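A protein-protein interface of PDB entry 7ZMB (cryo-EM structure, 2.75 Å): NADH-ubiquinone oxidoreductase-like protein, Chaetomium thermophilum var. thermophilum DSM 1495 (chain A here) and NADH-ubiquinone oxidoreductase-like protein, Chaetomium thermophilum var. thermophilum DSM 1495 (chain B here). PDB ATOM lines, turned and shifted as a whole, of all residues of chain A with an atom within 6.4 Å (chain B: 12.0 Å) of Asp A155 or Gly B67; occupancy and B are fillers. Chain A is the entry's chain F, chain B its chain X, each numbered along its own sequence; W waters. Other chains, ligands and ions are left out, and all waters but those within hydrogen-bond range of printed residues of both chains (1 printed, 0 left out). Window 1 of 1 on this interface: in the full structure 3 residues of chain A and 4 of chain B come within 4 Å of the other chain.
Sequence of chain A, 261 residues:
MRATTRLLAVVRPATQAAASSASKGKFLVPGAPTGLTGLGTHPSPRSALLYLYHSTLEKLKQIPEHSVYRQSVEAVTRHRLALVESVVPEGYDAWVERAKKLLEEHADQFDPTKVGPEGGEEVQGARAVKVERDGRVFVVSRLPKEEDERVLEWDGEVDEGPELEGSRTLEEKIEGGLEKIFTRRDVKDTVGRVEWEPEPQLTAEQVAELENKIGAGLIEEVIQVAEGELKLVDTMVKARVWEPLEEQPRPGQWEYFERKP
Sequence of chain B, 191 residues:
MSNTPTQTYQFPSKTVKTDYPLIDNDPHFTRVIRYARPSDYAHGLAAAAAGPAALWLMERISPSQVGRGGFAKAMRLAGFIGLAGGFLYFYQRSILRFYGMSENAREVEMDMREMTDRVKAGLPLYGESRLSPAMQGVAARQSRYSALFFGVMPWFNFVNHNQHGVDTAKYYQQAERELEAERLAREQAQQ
OD1 of Asp A155 lies close to N of Arg B68, 3.3 Å away. The side-chain carboxylate of Glu A149 lies within hydrogen-bond range of the backbone NH of Gly B69 (3.1 Å).
Among the printed residues, merely in contact across the chains: Glu A149 with Arg B68 (3.1 Å), Trp A154 with Gln B65 (3.4 Å) and Asp A155 with Gly B67 (3.3 Å).
Asp A155 touches two residues of chain B. Printed residues of chain A within 4 Å of Gly B67: Asp A155 (3.3 Å). Leu A152 touches none of the printed residues of chain B. Printed residues of chain A within 4 Å of Gln B65: Trp A154. Of the printed residues of chain A, Gly B69 touches Glu A149 (3.1 Å). Printed residues of chain B within 4 Å of Glu A149: Arg B68 (3.1 Å) and Gly B69 (3.1 Å). Phe B71 touches none of the printed residues of chain A. The nearest residue of chain A that does not touch Gly B67 is Trp A154 (4.4 Å). The nearest printed residue of chain A that does not touch Gln B65 is Lys A188 (4.6 Å).
Printed residues of chain B that touch a printed residue of chain A: Gln B65, Gly B67, Arg B68 and Gly B69. Of the 11 printed residues of chain A, 3 touch a printed residue of chain B. Printed residues of chain A that touch a printed residue of chain B: Glu A149, Trp A154 and Asp A155. Hydrophobic or aromatic side chains of chain A that line the printed part of chain B: Trp A154.
Water W1 lies within hydrogen-bond range of O of Ser B64 (2.9 Å), NE1 of Trp A154 (3.0 Å), O of Gln B65 (3.1 Å) and N of Val B66 (3.4 Å).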
ATOM      1  N   GLN A 124       3.239   7.975  16.419  1.00  0.00           N
ATOM      2  CA  GLN A 124       3.006   7.446  17.755  1.00  0.00           C
ATOM      3  C   GLN A 124       2.815   5.932  17.773  1.00  0.00           C
ATOM      4  O   GLN A 124       2.652   5.354  18.852  1.00  0.00           O
ATOM      5  CB  GLN A 124       1.797   8.150  18.371  1.00  0.00           C
ATOM      6  CG  GLN A 124       0.500   7.734  17.751  1.00  0.00           C
ATOM      7  CD  GLN A 124       0.128   8.604  16.581  1.00  0.00           C
ATOM      8  OE1 GLN A 124       0.779   8.567  15.541  1.00  0.00           O
ATOM      9  NE2 GLN A 124      -0.947   9.357  16.723  1.00  0.00           N
ATOM     10  N   GLY A 125       2.814   5.282  16.610  1.00  0.00           N
ATOM     11  CA  GLY A 125       2.938   3.847  16.515  1.00  0.00           C
ATOM     12  C   GLY A 125       4.215   3.455  15.789  1.00  0.00           C
ATOM     13  O   GLY A 125       5.000   4.300  15.361  1.00  0.00           O
ATOM     14  N   PRO A 144       8.192   4.638  18.049  1.00  0.00           N
ATOM     15  CA  PRO A 144       7.793   5.941  18.594  1.00  0.00           C
ATOM     16  C   PRO A 144       8.625   6.303  19.814  1.00  0.00           C
ATOM     17  O   PRO A 144       8.954   5.449  20.639  1.00  0.00           O
ATOM     18  CB  PRO A 144       6.315   5.741  18.952  1.00  0.00           C
ATOM     19  CG  PRO A 144       6.136   4.270  19.058  1.00  0.00           C
ATOM     20  CD  PRO A 144       7.090   3.664  18.072  1.00  0.00           C
ATOM     21  N   GLU A 149       5.139   8.900  30.767  1.00  0.00           N
ATOM     22  CA  GLU A 149       3.688   8.877  30.612  1.00  0.00           C
ATOM     23  C   GLU A 149       3.073  10.229  30.943  1.00  0.00           C
ATOM     24  O   GLU A 149       2.169  10.701  30.247  1.00  0.00           O
ATOM     25  CB  GLU A 149       3.104   7.797  31.519  1.00  0.00           C
ATOM     26  CG  GLU A 149       3.225   6.399  30.976  1.00  0.00           C
ATOM     27  CD  GLU A 149       2.010   6.001  30.183  1.00  0.00           C
ATOM     28  OE1 GLU A 149       0.911   6.484  30.525  1.00  0.00           O
ATOM     29  OE2 GLU A 149       2.157   5.209  29.229  1.00  0.00           O
ATOM     30  N   LEU A 152       3.175  12.971  28.138  1.00  0.00           N
ATOM     31  CA  LEU A 152       2.866  12.466  26.805  1.00  0.00           C
ATOM     32  C   LEU A 152       1.379  12.631  26.543  1.00  0.00           C
ATOM     33  O   LEU A 152       0.558  11.924  27.136  1.00  0.00           O
ATOM     34  CB  LEU A 152       3.284  11.005  26.659  1.00  0.00           C
ATOM     35  CG  LEU A 152       3.282  10.474  25.231  1.00  0.00           C
ATOM     36  CD1 LEU A 152       4.292  11.223  24.405  1.00  0.00           C
ATOM     37  CD2 LEU A 152       3.572   8.997  25.228  1.00  0.00           C
ATOM     38  N   GLU A 153       1.053  13.544  25.621  1.00  0.00           N
ATOM     39  CA  GLU A 153      -0.369  13.879  25.349  1.00  0.00           C
ATOM     40  C   GLU A 153      -0.873  13.081  24.152  1.00  0.00           C
ATOM     41  O   GLU A 153      -0.154  13.041  23.141  1.00  0.00           O
ATOM     42  CB  GLU A 153      -0.540  15.378  25.123  1.00  0.00           C
ATOM     43  CG  GLU A 153      -0.147  16.229  26.309  1.00  0.00           C
ATOM     44  CD  GLU A 153      -0.078  17.697  25.940  1.00  0.00           C
ATOM     45  OE1 GLU A 153       0.197  18.524  26.828  1.00  0.00           O
ATOM     46  OE2 GLU A 153      -0.299  18.002  24.756  1.00  0.00           O
ATOM     47  N   TRP A 154      -2.045  12.458  24.279  1.00  0.00           N
ATOM     48  CA  TRP A 154      -2.675  11.682  23.177  1.00  0.00           C
ATOM     49  C   TRP A 154      -1.754  10.575  22.656  1.00  0.00           C
ATOM     50  O   TRP A 154      -1.722  10.396  21.435  1.00  0.00           O
ATOM     51  CB  TRP A 154      -3.162  12.611  22.065  1.00  0.00           C
ATOM     52  CG  TRP A 154      -4.168  13.615  22.536  1.00  0.00           C
ATOM     53  CD1 TRP A 154      -5.449  13.366  22.931  1.00  0.00           C
ATOM     54  CD2 TRP A 154      -3.979  15.035  22.669  1.00  0.00           C
ATOM     55  NE1 TRP A 154      -6.073  14.529  23.287  1.00  0.00           N
ATOM     56  CE2 TRP A 154      -5.198  15.570  23.136  1.00  0.00           C
ATOM     57  CE3 TRP A 154      -2.910  15.904  22.429  1.00  0.00           C
ATOM     58  CZ2 TRP A 154      -5.368  16.932  23.376  1.00  0.00           C
ATOM     59  CZ3 TRP A 154      -3.080  17.249  22.666  1.00  0.00           C
ATOM     60  CH2 TRP A 154      -4.292  17.751  23.136  1.00  0.00           C
ATOM     61  N   ASP A 155      -1.006   9.911  23.542  1.00  0.00           N
ATOM     62  CA  ASP A 155      -0.119   8.783  23.156  1.00  0.00           C
ATOM     63  C   ASP A 155       1.066   9.293  22.341  1.00  0.00           C
ATOM     64  O   ASP A 155       1.806   8.449  21.810  1.00  0.00           O
ATOM     65  CB  ASP A 155      -0.873   7.675  22.416  1.00  0.00           C
ATOM     66  CG  ASP A 155      -1.983   7.049  23.241  1.00  0.00           C
ATOM     67  OD1 ASP A 155      -1.797   6.916  24.463  1.00  0.00           O
ATOM     68  OD2 ASP A 155      -3.028   6.713  22.654  1.00  0.00           O
ATOM     69  N   GLY A 156       1.263  10.609  22.267  1.00  0.00           N
ATOM     70  CA  GLY A 156       2.294  11.109  21.386  1.00  0.00           C
ATOM     71  C   GLY A 156       1.822  11.473  20.003  1.00  0.00           C
ATOM     72  O   GLY A 156       2.653  11.644  19.107  1.00  0.00           O
ATOM     73  N   GLU A 157       0.510  11.586  19.800  1.00  0.00           N
ATOM     74  CA  GLU A 157      -0.040  11.985  18.477  1.00  0.00           C
ATOM     75  C   GLU A 157       0.588  13.306  18.021  1.00  0.00           C
ATOM     76  O   GLU A 157       0.971  14.100  18.879  1.00  0.00           O
ATOM     77  CB  GLU A 157      -1.566  11.999  18.543  1.00  0.00           C
ATOM     78  CG  GLU A 157      -2.247  12.198  17.202  1.00  0.00           C
ATOM     79  CD  GLU A 157      -3.633  11.591  17.120  1.00  0.00           C
ATOM     80  OE1 GLU A 157      -4.208  11.284  18.183  1.00  0.00           O
ATOM     81  OE2 GLU A 157      -4.124  11.405  15.991  1.00  0.00           O
ATOM     82  N   LYS A 188      -4.620   1.951  17.280  1.00  0.00           N
ATOM     83  CA  LYS A 188      -5.130   0.718  17.858  1.00  0.00           C
ATOM     84  C   LYS A 188      -5.767  -0.198  16.821  1.00  0.00           C
ATOM     85  O   LYS A 188      -6.006  -1.371  17.120  1.00  0.00           O
ATOM     86  CB  LYS A 188      -6.136   1.044  18.963  1.00  0.00           C
ATOM     87  CG  LYS A 188      -5.548   1.844  20.109  1.00  0.00           C
ATOM     88  CD  LYS A 188      -6.629   2.337  21.056  1.00  0.00           C
ATOM     89  CE  LYS A 188      -7.517   3.379  20.387  1.00  0.00           C
ATOM     90  NZ  LYS A 188      -6.757   4.591  19.987  1.00  0.00           N
ATOM     91  N   GLU B  59     -16.960   7.171  30.010  1.00  0.00           N
ATOM     92  CA  GLU B  59     -15.815   6.603  29.258  1.00  0.00           C
ATOM     93  C   GLU B  59     -16.300   5.474  28.358  1.00  0.00           C
ATOM     94  O   GLU B  59     -15.831   5.407  27.213  1.00  0.00           O
ATOM     95  CB  GLU B  59     -14.741   6.084  30.211  1.00  0.00           C
ATOM     96  CG  GLU B  59     -13.406   5.849  29.525  1.00  0.00           C
ATOM     97  CD  GLU B  59     -12.799   7.076  28.865  1.00  0.00           C
ATOM     98  OE1 GLU B  59     -13.014   8.192  29.371  1.00  0.00           O
ATOM     99  OE2 GLU B  59     -12.112   6.910  27.843  1.00  0.00           O
ATOM    100  N   SER B  62     -18.830   7.119  25.610  1.00  0.00           N
ATOM    101  CA  SER B  62     -18.202   8.203  24.805  1.00  0.00           C
ATOM    102  C   SER B  62     -16.738   8.377  25.210  1.00  0.00           C
ATOM    103  O   SER B  62     -16.449   9.295  25.960  1.00  0.00           O
ATOM    104  CB  SER B  62     -18.990   9.479  24.932  1.00  0.00           C
ATOM    105  OG  SER B  62     -19.245   9.790  26.291  1.00  0.00           O
ATOM    106  N   PRO B  63     -15.756   7.550  24.758  1.00  0.00           N
ATOM    107  CA  PRO B  63     -14.364   7.780  25.180  1.00  0.00           C
ATOM    108  C   PRO B  63     -13.721   9.168  25.051  1.00  0.00           C
ATOM    109  O   PRO B  63     -13.971   9.844  24.093  1.00  0.00           O
ATOM    110  CB  PRO B  63     -13.581   6.762  24.345  1.00  0.00           C
ATOM    111  CG  PRO B  63     -14.569   5.665  24.058  1.00  0.00           C
ATOM    112  CD  PRO B  63     -15.873   6.396  23.843  1.00  0.00           C
ATOM    113  N   SER B  64     -12.812   9.493  25.965  1.00  0.00           N
ATOM    114  CA  SER B  64     -12.133  10.809  25.959  1.00  0.00           C
ATOM    115  C   SER B  64     -10.954  10.793  24.983  1.00  0.00           C
ATOM    116  O   SER B  64     -10.448  11.883  24.694  1.00  0.00           O
ATOM    117  CB  SER B  64     -11.671  11.096  27.356  1.00  0.00           C
ATOM    118  OG  SER B  64     -11.163   9.917  27.958  1.00  0.00           O
ATOM    119  N   GLN B  65     -10.528   9.609  24.527  1.00  0.00           N
ATOM    120  CA  GLN B  65      -9.344   9.456  23.632  1.00  0.00           C
ATOM    121  C   GLN B  65      -8.107   9.966  24.369  1.00  0.00           C
ATOM    122  O   GLN B  65      -7.218  10.509  23.708  1.00  0.00           O
ATOM    123  CB  GLN B  65      -9.578  10.125  22.273  1.00  0.00           C
ATOM    124  CG  GLN B  65     -10.910   9.769  21.630  1.00  0.00           C
ATOM    125  CD  GLN B  65     -11.054   8.292  21.358  1.00  0.00           C
ATOM    126  OE1 GLN B  65     -12.082   7.689  21.647  1.00  0.00           O
ATOM    127  NE2 GLN B  65     -10.016   7.697  20.793  1.00  0.00           N
ATOM    128  N   VAL B  66      -8.064   9.777  25.687  1.00  0.00           N
ATOM    129  CA  VAL B  66      -6.930  10.253  26.531  1.00  0.00           C
ATOM    130  C   VAL B  66      -5.720   9.343  26.315  1.00  0.00           C
ATOM    131  O   VAL B  66      -5.907   8.246  25.767  1.00  0.00           O
ATOM    132  CB  VAL B  66      -7.354  10.339  28.013  1.00  0.00           C
ATOM    133  CG1 VAL B  66      -7.609   8.976  28.630  1.00  0.00           C
ATOM    134  CG2 VAL B  66      -6.399  11.163  28.863  1.00  0.00           C
ATOM    135  N   GLY B  67      -4.527   9.800  26.701  1.00  0.00           N
ATOM    136  CA  GLY B  67      -3.303   8.986  26.603  1.00  0.00           C
ATOM    137  C   GLY B  67      -3.341   7.687  27.381  1.00  0.00           C
ATOM    138  O   GLY B  67      -4.423   7.245  27.734  1.00  0.00           O
ATOM    139  N   ARG B  68      -2.187   7.116  27.700  1.00  0.00           N
ATOM    140  CA  ARG B  68      -2.098   5.793  28.312  1.00  0.00           C
ATOM    141  C   ARG B  68      -2.371   5.772  29.810  1.00  0.00           C
ATOM    142  O   ARG B  68      -2.766   4.724  30.330  1.00  0.00           O
ATOM    143  CB  ARG B  68      -0.716   5.193  28.066  1.00  0.00           C
ATOM    144  CG  ARG B  68      -0.380   4.942  26.608  1.00  0.00           C
ATOM    145  CD  ARG B  68       0.823   4.023  26.464  1.00  0.00           C
ATOM    146  NE  ARG B  68       1.393   4.073  25.121  1.00  0.00           N
ATOM    147  CZ  ARG B  68       0.886   3.441  24.067  1.00  0.00           C
ATOM    148  NH1 ARG B  68      -0.207   2.702  24.196  1.00  0.00           N
ATOM    149  NH2 ARG B  68       1.473   3.546  22.883  1.00  0.00           N
ATOM    150  N   GLY B  69      -2.161   6.871  30.524  1.00  0.00           N
ATOM    151  CA  GLY B  69      -2.357   6.811  31.960  1.00  0.00           C
ATOM    152  C   GLY B  69      -3.230   7.911  32.521  1.00  0.00           C
ATOM    153  O   GLY B  69      -3.238   8.157  33.730  1.00  0.00           O
ATOM    154  N   GLY B  70      -3.979   8.577  31.641  1.00  0.00           N
ATOM    155  CA  GLY B  70      -4.794   9.697  32.067  1.00  0.00           C
ATOM    156  C   GLY B  70      -6.098   9.305  32.718  1.00  0.00           C
ATOM    157  O   GLY B  70      -6.566  10.002  33.622  1.00  0.00           O
ATOM    158  N   PHE B  71      -6.711   8.205  32.277  1.00  0.00           N
ATOM    159  CA  PHE B  71      -8.004   7.836  32.842  1.00  0.00           C
ATOM    160  C   PHE B  71      -7.863   7.337  34.270  1.00  0.00           C
ATOM    161  O   PHE B  71      -8.707   7.638  35.120  1.00  0.00           O
ATOM    162  CB  PHE B  71      -8.709   6.788  31.987  1.00  0.00           C
ATOM    163  CG  PHE B  71     -10.077   6.458  32.485  1.00  0.00           C
ATOM    164  CD1 PHE B  71     -11.133   7.318  32.249  1.00  0.00           C
ATOM    165  CD2 PHE B  71     -10.300   5.327  33.247  1.00  0.00           C
ATOM    166  CE1 PHE B  71     -12.387   7.042  32.738  1.00  0.00           C
ATOM    167  CE2 PHE B  71     -11.560   5.051  33.737  1.00  0.00           C
ATOM    168  CZ  PHE B  71     -12.599   5.905  33.478  1.00  0.00           C
ATOM    169  N   ALA B  72      -6.804   6.578  34.555  1.00  0.00           N
ATOM    170  CA  ALA B  72      -6.541   6.159  35.925  1.00  0.00           C
ATOM    171  C   ALA B  72      -6.327   7.363  36.831  1.00  0.00           C
ATOM    172  O   ALA B  72      -6.746   7.357  37.993  1.00  0.00           O
ATOM    173  CB  ALA B  72      -5.329   5.229  35.966  1.00  0.00           C
ATOM    174  N   LYS B  73      -5.679   8.407  36.315  1.00  0.00           N
ATOM    175  CA  LYS B  73      -5.560   9.648  37.068  1.00  0.00           C
ATOM    176  C   LYS B  73      -6.928  10.265  37.338  1.00  0.00           C
ATOM    177  O   LYS B  73      -7.202  10.715  38.455  1.00  0.00           O
ATOM    178  CB  LYS B  73      -4.664  10.629  36.317  1.00  0.00           C
ATOM    179  CG  LYS B  73      -4.598  12.003  36.942  1.00  0.00           C
ATOM    180  CD  LYS B  73      -3.873  12.992  36.065  1.00  0.00           C
ATOM    181  CE  LYS B  73      -3.633  14.296  36.814  1.00  0.00           C
ATOM    182  NZ  LYS B  73      -2.256  14.417  37.368  1.00  0.00           N
ATOM    183  N   ALA B  74      -7.802  10.289  36.329  1.00  0.00           N
ATOM    184  CA  ALA B  74      -9.120  10.891  36.497  1.00  0.00           C
ATOM    185  C   ALA B  74      -9.995  10.078  37.441  1.00  0.00           C
ATOM    186  O   ALA B  74     -10.843  10.643  38.137  1.00  0.00           O
ATOM    187  CB  ALA B  74      -9.805  11.047  35.140  1.00  0.00           C
ATOM    188  N   MET B  75      -9.810   8.758  37.472  1.00  0.00           N
ATOM    189  CA  MET B  75     -10.544   7.929  38.418  1.00  0.00           C
ATOM    190  C   MET B  75     -10.197   8.291  39.852  1.00  0.00           C
ATOM    191  O   MET B  75     -11.079   8.367  40.713  1.00  0.00           O
ATOM    192  CB  MET B  75     -10.250   6.455  38.151  1.00  0.00           C
ATOM    193  CG  MET B  75     -11.236   5.766  37.251  1.00  0.00           C
ATOM    194  SD  MET B  75     -12.889   5.665  37.953  1.00  0.00           S
ATOM    195  CE  MET B  75     -13.769   6.786  36.896  1.00  0.00           C
ATOM    196  N   ARG B  76      -8.916   8.535  40.120  1.00  0.00           N
ATOM    197  CA  ARG B  76      -8.485   8.889  41.466  1.00  0.00           C
ATOM    198  C   ARG B  76      -9.122  10.190  41.936  1.00  0.00           C
ATOM    199  O   ARG B  76      -9.477  10.321  43.110  1.00  0.00           O
ATOM    200  CB  ARG B  76      -6.964   8.985  41.512  1.00  0.00           C
ATOM    201  CG  ARG B  76      -6.274   7.646  41.650  1.00  0.00           C
ATOM    202  CD  ARG B  76      -4.832   7.829  42.014  1.00  0.00           C
ATOM    203  NE  ARG B  76      -4.096   8.463  40.931  1.00  0.00           N
ATOM    204  CZ  ARG B  76      -3.518   7.809  39.931  1.00  0.00           C
ATOM    205  NH1 ARG B  76      -3.578   6.490  39.870  1.00  0.00           N
ATOM    206  NH2 ARG B  76      -2.871   8.481  38.996  1.00  0.00           N
HETATM  207  O   HOH W   1      -7.830  13.094  25.233  1.00  0.00           O
